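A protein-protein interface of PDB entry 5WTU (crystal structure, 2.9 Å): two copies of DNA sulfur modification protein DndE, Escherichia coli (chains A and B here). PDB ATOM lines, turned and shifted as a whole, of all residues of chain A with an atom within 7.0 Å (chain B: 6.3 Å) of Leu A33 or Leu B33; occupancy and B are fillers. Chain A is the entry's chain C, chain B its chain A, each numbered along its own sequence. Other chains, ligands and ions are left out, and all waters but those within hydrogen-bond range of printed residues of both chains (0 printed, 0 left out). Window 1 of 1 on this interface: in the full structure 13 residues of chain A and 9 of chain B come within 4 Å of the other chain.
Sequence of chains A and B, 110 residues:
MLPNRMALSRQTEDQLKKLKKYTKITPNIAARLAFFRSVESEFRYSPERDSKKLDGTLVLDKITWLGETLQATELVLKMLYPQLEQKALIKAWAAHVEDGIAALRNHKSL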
ATOM      1  N   ILE A  25     -16.245 -27.029   5.600  1.00  0.00           N
ATOM      2  CA  ILE A  25     -16.851 -28.337   5.862  1.00  0.00           C
ATOM      3  C   ILE A  25     -16.340 -28.976   7.163  1.00  0.00           C
ATOM      4  O   ILE A  25     -17.096 -29.671   7.848  1.00  0.00           O
ATOM      5  CB  ILE A  25     -16.716 -29.303   4.641  1.00  0.00           C
ATOM      6  CG1 ILE A  25     -17.746 -30.444   4.706  1.00  0.00           C
ATOM      7  CG2 ILE A  25     -15.302 -29.853   4.506  1.00  0.00           C
ATOM      8  CD1 ILE A  25     -18.036 -31.126   3.377  1.00  0.00           C
ATOM      9  N   THR A  26     -15.073 -28.726   7.504  1.00  0.00           N
ATOM     10  CA  THR A  26     -14.443 -29.354   8.672  1.00  0.00           C
ATOM     11  C   THR A  26     -14.664 -28.520   9.940  1.00  0.00           C
ATOM     12  O   THR A  26     -14.551 -27.291   9.885  1.00  0.00           O
ATOM     13  CB  THR A  26     -12.930 -29.604   8.463  1.00  0.00           C
ATOM     14  OG1 THR A  26     -12.253 -28.354   8.285  1.00  0.00           O
ATOM     15  CG2 THR A  26     -12.672 -30.521   7.259  1.00  0.00           C
ATOM     16  N   ASN A  28     -13.323 -27.283  12.717  1.00  0.00           N
ATOM     17  CA  ASN A  28     -12.507 -26.150  13.174  1.00  0.00           C
ATOM     18  C   ASN A  28     -12.591 -24.898  12.299  1.00  0.00           C
ATOM     19  O   ASN A  28     -12.741 -23.793  12.821  1.00  0.00           O
ATOM     20  CB  ASN A  28     -11.045 -26.570  13.410  1.00  0.00           C
ATOM     21  CG  ASN A  28     -10.424 -27.284  12.218  1.00  0.00           C
ATOM     22  OD1 ASN A  28     -11.083 -28.047  11.508  1.00  0.00           O
ATOM     23  ND2 ASN A  28      -9.136 -27.055  12.010  1.00  0.00           N
ATOM     24  N   ILE A  29     -12.500 -25.077  10.981  1.00  0.00           N
ATOM     25  CA  ILE A  29     -12.683 -23.983  10.018  1.00  0.00           C
ATOM     26  C   ILE A  29     -14.105 -23.437  10.135  1.00  0.00           C
ATOM     27  O   ILE A  29     -14.307 -22.219  10.183  1.00  0.00           O
ATOM     28  CB  ILE A  29     -12.400 -24.433   8.567  1.00  0.00           C
ATOM     29  CG1 ILE A  29     -10.950 -24.900   8.420  1.00  0.00           C
ATOM     30  CG2 ILE A  29     -12.694 -23.309   7.576  1.00  0.00           C
ATOM     31  CD1 ILE A  29     -10.682 -25.690   7.157  1.00  0.00           C
ATOM     32  N   ALA A  30     -15.073 -24.354  10.201  1.00  0.00           N
ATOM     33  CA  ALA A  30     -16.483 -24.025  10.411  1.00  0.00           C
ATOM     34  C   ALA A  30     -16.686 -23.181  11.672  1.00  0.00           C
ATOM     35  O   ALA A  30     -17.478 -22.236  11.662  1.00  0.00           O
ATOM     36  CB  ALA A  30     -17.319 -25.295  10.474  1.00  0.00           C
ATOM     37  N   ALA A  31     -15.954 -23.523  12.736  1.00  0.00           N
ATOM     38  CA  ALA A  31     -15.969 -22.780  13.997  1.00  0.00           C
ATOM     39  C   ALA A  31     -15.430 -21.356  13.842  1.00  0.00           C
ATOM     40  O   ALA A  31     -15.959 -20.425  14.458  1.00  0.00           O
ATOM     41  CB  ALA A  31     -15.196 -23.535  15.073  1.00  0.00           C
ATOM     42  N   ARG A  32     -14.392 -21.200  13.016  1.00  0.00           N
ATOM     43  CA  ARG A  32     -13.782 -19.894  12.744  1.00  0.00           C
ATOM     44  C   ARG A  32     -14.725 -19.017  11.940  1.00  0.00           C
ATOM     45  O   ARG A  32     -14.920 -17.846  12.269  1.00  0.00           O
ATOM     46  CB  ARG A  32     -12.458 -20.049  12.000  1.00  0.00           C
ATOM     47  CG  ARG A  32     -11.398 -20.817  12.761  1.00  0.00           C
ATOM     48  CD  ARG A  32     -10.278 -21.246  11.834  1.00  0.00           C
ATOM     49  NE  ARG A  32      -9.528 -22.372  12.387  1.00  0.00           N
ATOM     50  CZ  ARG A  32      -8.421 -22.888  11.860  1.00  0.00           C
ATOM     51  NH1 ARG A  32      -7.893 -22.382  10.752  1.00  0.00           N
ATOM     52  NH2 ARG A  32      -7.830 -23.913  12.454  1.00  0.00           N
ATOM     53  N   LEU A  33     -15.311 -19.600  10.893  1.00  0.00           N
ATOM     54  CA  LEU A  33     -16.280 -18.910  10.040  1.00  0.00           C
ATOM     55  C   LEU A  33     -17.508 -18.482  10.829  1.00  0.00           C
ATOM     56  O   LEU A  33     -17.977 -17.356  10.667  1.00  0.00           O
ATOM     57  CB  LEU A  33     -16.685 -19.785   8.852  1.00  0.00           C
ATOM     58  CG  LEU A  33     -15.604 -20.110   7.816  1.00  0.00           C
ATOM     59  CD1 LEU A  33     -15.948 -21.386   7.068  1.00  0.00           C
ATOM     60  CD2 LEU A  33     -15.417 -18.965   6.839  1.00  0.00           C
ATOM     61  N   ALA A  34     -17.995 -19.375  11.695  1.00  0.00           N
ATOM     62  CA  ALA A  34     -19.150 -19.110  12.558  1.00  0.00           C
ATOM     63  C   ALA A  34     -18.866 -18.013  13.577  1.00  0.00           C
ATOM     64  O   ALA A  34     -19.693 -17.124  13.771  1.00  0.00           O
ATOM     65  CB  ALA A  34     -19.613 -20.384  13.250  1.00  0.00           C
ATOM     66  N   PHE A  35     -17.689 -18.072  14.205  1.00  0.00           N
ATOM     67  CA  PHE A  35     -17.256 -17.063  15.179  1.00  0.00           C
ATOM     68  C   PHE A  35     -17.252 -15.648  14.582  1.00  0.00           C
ATOM     69  O   PHE A  35     -17.894 -14.744  15.127  1.00  0.00           O
ATOM     70  CB  PHE A  35     -15.873 -17.420  15.752  1.00  0.00           C
ATOM     71  CG  PHE A  35     -15.351 -16.431  16.759  1.00  0.00           C
ATOM     72  CD1 PHE A  35     -14.616 -15.312  16.348  1.00  0.00           C
ATOM     73  CD2 PHE A  35     -15.572 -16.623  18.121  1.00  0.00           C
ATOM     74  CE1 PHE A  35     -14.134 -14.397  17.277  1.00  0.00           C
ATOM     75  CE2 PHE A  35     -15.089 -15.713  19.056  1.00  0.00           C
ATOM     76  CZ  PHE A  35     -14.371 -14.596  18.633  1.00  0.00           C
ATOM     77  N   PHE A  36     -16.538 -15.473  13.468  1.00  0.00           N
ATOM     78  CA  PHE A  36     -16.390 -14.158  12.837  1.00  0.00           C
ATOM     79  C   PHE A  36     -17.676 -13.643  12.195  1.00  0.00           C
ATOM     80  O   PHE A  36     -17.886 -12.431  12.119  1.00  0.00           O
ATOM     81  CB  PHE A  36     -15.211 -14.146  11.863  1.00  0.00           C
ATOM     82  CG  PHE A  36     -13.874 -14.158  12.548  1.00  0.00           C
ATOM     83  CD1 PHE A  36     -13.294 -12.969  12.993  1.00  0.00           C
ATOM     84  CD2 PHE A  36     -13.202 -15.356  12.780  1.00  0.00           C
ATOM     85  CE1 PHE A  36     -12.062 -12.977  13.639  1.00  0.00           C
ATOM     86  CE2 PHE A  36     -11.969 -15.371  13.419  1.00  0.00           C
ATOM     87  CZ  PHE A  36     -11.398 -14.179  13.851  1.00  0.00           C
ATOM     88  N   ARG A  37     -18.522 -14.568  11.743  1.00  0.00           N
ATOM     89  CA  ARG A  37     -19.884 -14.256  11.299  1.00  0.00           C
ATOM     90  C   ARG A  37     -20.708 -13.663  12.446  1.00  0.00           C
ATOM     91  O   ARG A  37     -21.420 -12.668  12.259  1.00  0.00           O
ATOM     92  CB  ARG A  37     -20.558 -15.522  10.742  1.00  0.00           C
ATOM     93  CG  ARG A  37     -22.048 -15.420  10.452  1.00  0.00           C
ATOM     94  CD  ARG A  37     -22.347 -14.541   9.251  1.00  0.00           C
ATOM     95  NE  ARG A  37     -23.785 -14.331   9.088  1.00  0.00           N
ATOM     96  CZ  ARG A  37     -24.482 -13.350   9.661  1.00  0.00           C
ATOM     97  NH1 ARG A  37     -25.787 -13.255   9.441  1.00  0.00           N
ATOM     98  NH2 ARG A  37     -23.886 -12.464  10.454  1.00  0.00           N
ATOM     99  N   SER A  38     -20.587 -14.276  13.624  1.00  0.00           N
ATOM    100  CA  SER A  38     -21.304 -13.857  14.825  1.00  0.00           C
ATOM    101  C   SER A  38     -20.802 -12.540  15.397  1.00  0.00           C
ATOM    102  O   SER A  38     -21.594 -11.706  15.838  1.00  0.00           O
ATOM    103  CB  SER A  38     -21.191 -14.936  15.895  1.00  0.00           C
ATOM    104  OG  SER A  38     -21.651 -14.475  17.153  1.00  0.00           O
ATOM    105  N   GLU A  40     -19.226 -10.075  13.936  1.00  0.00           N
ATOM    106  CA  GLU A  40     -19.512  -8.947  13.056  1.00  0.00           C
ATOM    107  C   GLU A  40     -21.001  -8.582  13.056  1.00  0.00           C
ATOM    108  O   GLU A  40     -21.396  -7.567  12.479  1.00  0.00           O
ATOM    109  CB  GLU A  40     -19.009  -9.237  11.642  1.00  0.00           C
ATOM    110  CG  GLU A  40     -17.491  -9.153  11.506  1.00  0.00           C
ATOM    111  CD  GLU A  40     -16.937  -9.985  10.364  1.00  0.00           C
ATOM    112  OE1 GLU A  40     -17.720 -10.676   9.677  1.00  0.00           O
ATOM    113  OE2 GLU A  40     -15.705  -9.959  10.158  1.00  0.00           O
ATOM    114  N   THR A  69      -6.337 -17.803  12.733  1.00  0.00           N
ATOM    115  CA  THR A  69      -7.315 -16.851  13.272  1.00  0.00           C
ATOM    116  C   THR A  69      -7.121 -16.601  14.778  1.00  0.00           C
ATOM    117  O   THR A  69      -7.866 -15.825  15.380  1.00  0.00           O
ATOM    118  CB  THR A  69      -8.779 -17.264  12.969  1.00  0.00           C
ATOM    119  OG1 THR A  69      -9.164 -18.372  13.789  1.00  0.00           O
ATOM    120  CG2 THR A  69      -8.951 -17.634  11.507  1.00  0.00           C
ATOM    121  N   GLY A 100     -23.052 -18.068  15.733  1.00  0.00           N
ATOM    122  CA  GLY A 100     -22.580 -18.074  14.358  1.00  0.00           C
ATOM    123  C   GLY A 100     -23.181 -19.175  13.521  1.00  0.00           C
ATOM    124  O   GLY A 100     -23.656 -18.912  12.422  1.00  0.00           O
ATOM    125  N   ILE A 101     -23.157 -20.399  14.044  1.00  0.00           N
ATOM    126  CA  ILE A 101     -23.771 -21.551  13.378  1.00  0.00           C
ATOM    127  C   ILE A 101     -25.262 -21.300  13.173  1.00  0.00           C
ATOM    128  O   ILE A 101     -25.790 -21.568  12.097  1.00  0.00           O
ATOM    129  CB  ILE A 101     -23.543 -22.873  14.145  1.00  0.00           C
ATOM    130  CG1 ILE A 101     -22.050 -23.125  14.345  1.00  0.00           C
ATOM    131  CG2 ILE A 101     -24.149 -24.053  13.392  1.00  0.00           C
ATOM    132  CD1 ILE A 101     -21.731 -24.102  15.455  1.00  0.00           C
ATOM    133  N   LEU A 104     -25.638 -18.881  10.308  1.00  0.00           N
ATOM    134  CA  LEU A 104     -25.302 -19.538   9.045  1.00  0.00           C
ATOM    135  C   LEU A 104     -26.388 -20.512   8.605  1.00  0.00           C
ATOM    136  O   LEU A 104     -26.650 -20.658   7.412  1.00  0.00           O
ATOM    137  CB  LEU A 104     -23.955 -20.255   9.145  1.00  0.00           C
ATOM    138  CG  LEU A 104     -22.686 -19.408   9.277  1.00  0.00           C
ATOM    139  CD1 LEU A 104     -21.505 -20.297   9.628  1.00  0.00           C
ATOM    140  CD2 LEU A 104     -22.391 -18.601   8.020  1.00  0.00           C
ATOM    141  N   LEU B  19     -20.068 -24.366  -4.701  1.00  0.00           N
ATOM    142  CA  LEU B  19     -20.112 -24.566  -3.258  1.00  0.00           C
ATOM    143  C   LEU B  19     -21.558 -24.470  -2.800  1.00  0.00           C
ATOM    144  O   LEU B  19     -22.114 -23.381  -2.665  1.00  0.00           O
ATOM    145  CB  LEU B  19     -19.220 -23.565  -2.521  1.00  0.00           C
ATOM    146  CG  LEU B  19     -18.994 -23.812  -1.024  1.00  0.00           C
ATOM    147  CD1 LEU B  19     -18.033 -24.968  -0.782  1.00  0.00           C
ATOM    148  CD2 LEU B  19     -18.496 -22.553  -0.329  1.00  0.00           C
ATOM    149  N   TYR B  22     -22.398 -27.361   3.338  1.00  0.00           N
ATOM    150  CA  TYR B  22     -21.358 -27.204   4.358  1.00  0.00           C
ATOM    151  C   TYR B  22     -20.626 -28.506   4.680  1.00  0.00           C
ATOM    152  O   TYR B  22     -20.995 -29.582   4.206  1.00  0.00           O
ATOM    153  CB  TYR B  22     -21.952 -26.613   5.639  1.00  0.00           C
ATOM    154  CG  TYR B  22     -22.118 -25.113   5.611  1.00  0.00           C
ATOM    155  CD1 TYR B  22     -21.031 -24.272   5.866  1.00  0.00           C
ATOM    156  CD2 TYR B  22     -23.360 -24.528   5.336  1.00  0.00           C
ATOM    157  CE1 TYR B  22     -21.172 -22.890   5.843  1.00  0.00           C
ATOM    158  CE2 TYR B  22     -23.513 -23.145   5.317  1.00  0.00           C
ATOM    159  CZ  TYR B  22     -22.413 -22.334   5.565  1.00  0.00           C
ATOM    160  OH  TYR B  22     -22.544 -20.965   5.545  1.00  0.00           O
ATOM    161  N   ILE B  25     -25.739 -23.266   0.679  1.00  0.00           N
ATOM    162  CA  ILE B  25     -24.821 -22.131   0.486  1.00  0.00           C
ATOM    163  C   ILE B  25     -25.147 -21.338  -0.788  1.00  0.00           C
ATOM    164  O   ILE B  25     -25.311 -21.912  -1.869  1.00  0.00           O
ATOM    165  CB  ILE B  25     -23.330 -22.570   0.518  1.00  0.00           C
ATOM    166  CG1 ILE B  25     -22.926 -22.966   1.943  1.00  0.00           C
ATOM    167  CG2 ILE B  25     -22.411 -21.456   0.036  1.00  0.00           C
ATOM    168  CD1 ILE B  25     -21.573 -23.639   2.070  1.00  0.00           C
ATOM    169  N   THR B  26     -25.241 -20.015  -0.627  1.00  0.00           N
ATOM    170  CA  THR B  26     -25.506 -19.060  -1.714  1.00  0.00           C
ATOM    171  C   THR B  26     -24.215 -18.333  -2.155  1.00  0.00           C
ATOM    172  O   THR B  26     -23.324 -18.134  -1.324  1.00  0.00           O
ATOM    173  CB  THR B  26     -26.577 -18.029  -1.293  1.00  0.00           C
ATOM    174  OG1 THR B  26     -26.182 -17.391  -0.073  1.00  0.00           O
ATOM    175  CG2 THR B  26     -27.928 -18.706  -1.093  1.00  0.00           C
ATOM    176  N   ASN B  28     -22.936 -15.192  -2.872  1.00  0.00           N
ATOM    177  CA  ASN B  28     -22.367 -14.080  -2.098  1.00  0.00           C
ATOM    178  C   ASN B  28     -21.795 -14.509  -0.741  1.00  0.00           C
ATOM    179  O   ASN B  28     -20.738 -14.021  -0.328  1.00  0.00           O
ATOM    180  CB  ASN B  28     -23.376 -12.933  -1.937  1.00  0.00           C
ATOM    181  CG  ASN B  28     -24.692 -13.383  -1.326  1.00  0.00           C
ATOM    182  OD1 ASN B  28     -25.333 -14.323  -1.808  1.00  0.00           O
ATOM    183  ND2 ASN B  28     -25.106 -12.709  -0.260  1.00  0.00           N
ATOM    184  N   ILE B  29     -22.493 -15.430  -0.072  1.00  0.00           N
ATOM    185  CA  ILE B  29     -22.034 -16.023   1.191  1.00  0.00           C
ATOM    186  C   ILE B  29     -20.784 -16.876   0.955  1.00  0.00           C
ATOM    187  O   ILE B  29     -19.809 -16.754   1.698  1.00  0.00           O
ATOM    188  CB  ILE B  29     -23.154 -16.848   1.890  1.00  0.00           C
ATOM    189  CG1 ILE B  29     -24.403 -15.986   2.165  1.00  0.00           C
ATOM    190  CG2 ILE B  29     -22.648 -17.531   3.161  1.00  0.00           C
ATOM    191  CD1 ILE B  29     -24.227 -14.817   3.120  1.00  0.00           C
ATOM    192  N   ALA B  30     -20.819 -17.713  -0.088  1.00  0.00           N
ATOM    193  CA  ALA B  30     -19.660 -18.503  -0.521  1.00  0.00           C
ATOM    194  C   ALA B  30     -18.431 -17.621  -0.728  1.00  0.00           C
ATOM    195  O   ALA B  30     -17.329 -18.007  -0.346  1.00  0.00           O
ATOM    196  CB  ALA B  30     -19.978 -19.287  -1.788  1.00  0.00           C
ATOM    197  N   ALA B  31     -18.641 -16.437  -1.311  1.00  0.00           N
ATOM    198  CA  ALA B  31     -17.583 -15.445  -1.521  1.00  0.00           C
ATOM    199  C   ALA B  31     -16.991 -14.924  -0.214  1.00  0.00           C
ATOM    200  O   ALA B  31     -15.772 -14.768  -0.110  1.00  0.00           O
ATOM    201  CB  ALA B  31     -18.085 -14.293  -2.378  1.00  0.00           C
ATOM    202  N   ARG B  32     -17.852 -14.673   0.774  1.00  0.00           N
ATOM    203  CA  ARG B  32     -17.426 -14.183   2.094  1.00  0.00           C
ATOM    204  C   ARG B  32     -16.610 -15.225   2.848  1.00  0.00           C
ATOM    205  O   ARG B  32     -15.587 -14.900   3.463  1.00  0.00           O
ATOM    206  CB  ARG B  32     -18.626 -13.787   2.950  1.00  0.00           C
ATOM    207  CG  ARG B  32     -19.467 -12.663   2.394  1.00  0.00           C
ATOM    208  CD  ARG B  32     -20.732 -12.538   3.216  1.00  0.00           C
ATOM    209  NE  ARG B  32     -21.785 -11.845   2.484  1.00  0.00           N
ATOM    210  CZ  ARG B  32     -22.934 -11.440   3.015  1.00  0.00           C
ATOM    211  NH1 ARG B  32     -23.198 -11.644   4.303  1.00  0.00           N
ATOM    212  NH2 ARG B  32     -23.824 -10.817   2.255  1.00  0.00           N
ATOM    213  N   LEU B  33     -17.086 -16.469   2.797  1.00  0.00           N
ATOM    214  CA  LEU B  33     -16.409 -17.608   3.404  1.00  0.00           C
ATOM    215  C   LEU B  33     -15.059 -17.849   2.726  1.00  0.00           C
ATOM    216  O   LEU B  33     -14.075 -18.148   3.402  1.00  0.00           O
ATOM    217  CB  LEU B  33     -17.288 -18.867   3.350  1.00  0.00           C
ATOM    218  CG  LEU B  33     -18.724 -18.819   3.911  1.00  0.00           C
ATOM    219  CD1 LEU B  33     -19.587 -19.923   3.308  1.00  0.00           C
ATOM    220  CD2 LEU B  33     -18.771 -18.876   5.428  1.00  0.00           C
ATOM    221  N   ALA B  34     -15.027 -17.691   1.400  1.00  0.00           N
ATOM    222  CA  ALA B  34     -13.806 -17.854   0.599  1.00  0.00           C
ATOM    223  C   ALA B  34     -12.778 -16.763   0.857  1.00  0.00           C
ATOM    224  O   ALA B  34     -11.583 -17.050   0.942  1.00  0.00           O
ATOM    225  CB  ALA B  34     -14.138 -17.924  -0.882  1.00  0.00           C
ATOM    226  N   PHE B  35     -13.241 -15.518   0.977  1.00  0.00           N
ATOM    227  CA  PHE B  35     -12.349 -14.396   1.261  1.00  0.00           C
ATOM    228  C   PHE B  35     -11.656 -14.568   2.610  1.00  0.00           C
ATOM    229  O   PHE B  35     -10.434 -14.451   2.697  1.00  0.00           O
ATOM    230  CB  PHE B  35     -13.079 -13.052   1.202  1.00  0.00           C
ATOM    231  CG  PHE B  35     -12.182 -11.878   1.473  1.00  0.00           C
ATOM    232  CD1 PHE B  35     -11.352 -11.376   0.470  1.00  0.00           C
ATOM    233  CD2 PHE B  35     -12.143 -11.284   2.735  1.00  0.00           C
ATOM    234  CE1 PHE B  35     -10.509 -10.301   0.714  1.00  0.00           C
ATOM    235  CE2 PHE B  35     -11.300 -10.213   2.985  1.00  0.00           C
ATOM    236  CZ  PHE B  35     -10.484  -9.720   1.972  1.00  0.00           C
ATOM    237  N   PHE B  36     -12.447 -14.847   3.646  1.00  0.00           N
ATOM    238  CA  PHE B  36     -11.932 -15.062   4.995  1.00  0.00           C
ATOM    239  C   PHE B  36     -10.973 -16.259   5.062  1.00  0.00           C
ATOM    240  O   PHE B  36      -9.920 -16.172   5.698  1.00  0.00           O
ATOM    241  CB  PHE B  36     -13.095 -15.209   5.991  1.00  0.00           C
ATOM    242  CG  PHE B  36     -12.683 -15.730   7.343  1.00  0.00           C
ATOM    243  CD1 PHE B  36     -12.673 -17.103   7.599  1.00  0.00           C
ATOM    244  CD2 PHE B  36     -12.302 -14.856   8.358  1.00  0.00           C
ATOM    245  CE1 PHE B  36     -12.289 -17.594   8.836  1.00  0.00           C
ATOM    246  CE2 PHE B  36     -11.916 -15.341   9.596  1.00  0.00           C
ATOM    247  CZ  PHE B  36     -11.913 -16.711   9.835  1.00  0.00           C
ATOM    248  N   ARG B  37     -11.347 -17.358   4.402  1.00  0.00           N
ATOM    249  CA  ARG B  37     -10.534 -18.582   4.334  1.00  0.00           C
ATOM    250  C   ARG B  37      -9.169 -18.341   3.686  1.00  0.00           C
ATOM    251  O   ARG B  37      -8.162 -18.915   4.114  1.00  0.00           O
ATOM    252  CB  ARG B  37     -11.295 -19.692   3.590  1.00  0.00           C
ATOM    253  CG  ARG B  37     -10.598 -21.047   3.496  1.00  0.00           C
ATOM    254  CD  ARG B  37     -10.674 -21.832   4.796  1.00  0.00           C
ATOM    255  NE  ARG B  37     -10.061 -23.155   4.667  1.00  0.00           N
ATOM    256  CZ  ARG B  37      -8.804 -23.455   4.995  1.00  0.00           C
ATOM    257  NH1 ARG B  37      -8.359 -24.694   4.828  1.00  0.00           N
ATOM    258  NH2 ARG B  37      -7.986 -22.534   5.494  1.00  0.00           N
ATOM    259  N   SER B  38      -9.147 -17.502   2.651  1.00  0.00           N
ATOM    260  CA  SER B  38      -7.910 -17.151   1.955  1.00  0.00           C
ATOM    261  C   SER B  38      -7.044 -16.194   2.769  1.00  0.00           C
ATOM    262  O   SER B  38      -5.817 -16.293   2.746  1.00  0.00           O
ATOM    263  CB  SER B  38      -8.220 -16.529   0.602  1.00  0.00           C
ATOM    264  OG  SER B  38      -7.032 -16.223  -0.107  1.00  0.00           O
ATOM    265  N   GLU B  40      -7.039 -15.938   6.089  1.00  0.00           N
ATOM    266  CA  GLU B  40      -6.479 -16.760   7.162  1.00  0.00           C
ATOM    267  C   GLU B  40      -5.438 -17.779   6.664  1.00  0.00           C
ATOM    268  O   GLU B  40      -4.834 -18.484   7.464  1.00  0.00           O
ATOM    269  CB  GLU B  40      -7.582 -17.450   7.983  1.00  0.00           C
ATOM    270  CG  GLU B  40      -8.237 -18.655   7.313  1.00  0.00           C
ATOM    271  CD  GLU B  40      -8.515 -19.802   8.270  1.00  0.00           C
ATOM    272  OE1 GLU B  40      -7.589 -20.218   9.001  1.00  0.00           O
ATOM    273  OE2 GLU B  40      -9.660 -20.305   8.275  1.00  0.00           O
ATOM    274  N   GLY B 100      -9.573 -18.900  -1.913  1.00  0.00           N
ATOM    275  CA  GLY B 100     -10.385 -19.438  -0.829  1.00  0.00           C
ATOM    276  C   GLY B 100     -11.375 -20.497  -1.263  1.00  0.00           C
ATOM    277  O   GLY B 100     -11.504 -21.527  -0.598  1.00  0.00           O
ATOM    278  N   LEU B 104     -11.730 -24.288  -0.169  1.00  0.00           N
ATOM    279  CA  LEU B 104     -12.958 -24.815   0.437  1.00  0.00           C
ATOM    280  C   LEU B 104     -13.538 -26.060  -0.255  1.00  0.00           C
ATOM    281  O   LEU B 104     -14.544 -26.616   0.206  1.00  0.00           O
ATOM    282  CB  LEU B 104     -14.024 -23.712   0.556  1.00  0.00           C
ATOM    283  CG  LEU B 104     -13.834 -22.587   1.583  1.00  0.00           C
ATOM    284  CD1 LEU B 104     -14.790 -21.449   1.280  1.00  0.00           C
ATOM    285  CD2 LEU B 104     -14.026 -23.061   3.017  1.00  0.00           C
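The side-chain carboxylate (OE1) of Glu B40 lies within salt-bridge range of the guanidinium group (NH1) of Arg A32 (2.8 Å).
NH2 of Arg B37 lies within salt-bridge range of OE2 of Glu B40. NH2 of Arg A32 lies close to ND2 of Asn A28 (3.4 Å).
Among the printed residues, pairs that only touch across the chains: Ile A25 with Tyr B22 (3.4 Å), Ile A29 with Arg B37 (3.4 Å), Leu A33 with Leu B33 (3.6 Å), Leu A33 with Phe B36 (3.4 Å), Phe A36 with Phe B36 (3.4 Å), Thr A69 with Phe B36 (3.5 Å), Thr A69 with Glu B40 (3.8 Å) and Leu A104 with Tyr B22 (3.4 Å).
Of the printed residues of chain B, Ile A25 touches Tyr B22. Of the printed residues of chain B, Arg A32 touches Glu B40 (2.8 Å). Leu A33 touches two residues of chain B. Of the printed residues of chain B, Leu A104 touches Tyr B22 (3.4 Å). Leu B33 touches one residue of chain A. Printed residues of chain A within 4 Å of Glu B40: Arg A32 and Thr A69. The nearest residue of chain B that does not touch Leu A33 is Leu B104 (4.8 Å).
Of the 18 printed residues of chain A, 7 touch a printed residue of chain B. Printed residues of chain A that touch a printed residue of chain B: Ile A25, Ile A29, Arg A32, Leu A33, Phe A36, Thr A69 and Leu A104. Hydrophobic or aromatic side chains of chain A within 4 Å of the printed part of chain B: Ile A25, Ile A29, Leu A33, Phe A36 and Leu A104. Of the 18 printed residues of chain B, 5 touch a printed residue of chain A. Printed residues of chain B that touch a printed residue of chain A: Tyr B22, Leu B33, Phe B36, Arg B37 and Glu B40. Hydrophobic or aromatic side chains of chain B that line the printed part of chain A: Tyr B22, Leu B33 and Phe B36. Among the printed residues, 9 pairs touch across the chains.
Ile A29 touches Arg B37, but with the chains exchanged Arg A37 does not touch Ile B29 (6.0 Å). Arg A32 touches Glu B40, but with the chains exchanged Glu A40 does not touch Arg B32 (7.4 Å). Leu B33 touches its own counterpart, Leu A33. Phe A36 touches its own counterpart, Phe B36. 16 positions are printed for both chains.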
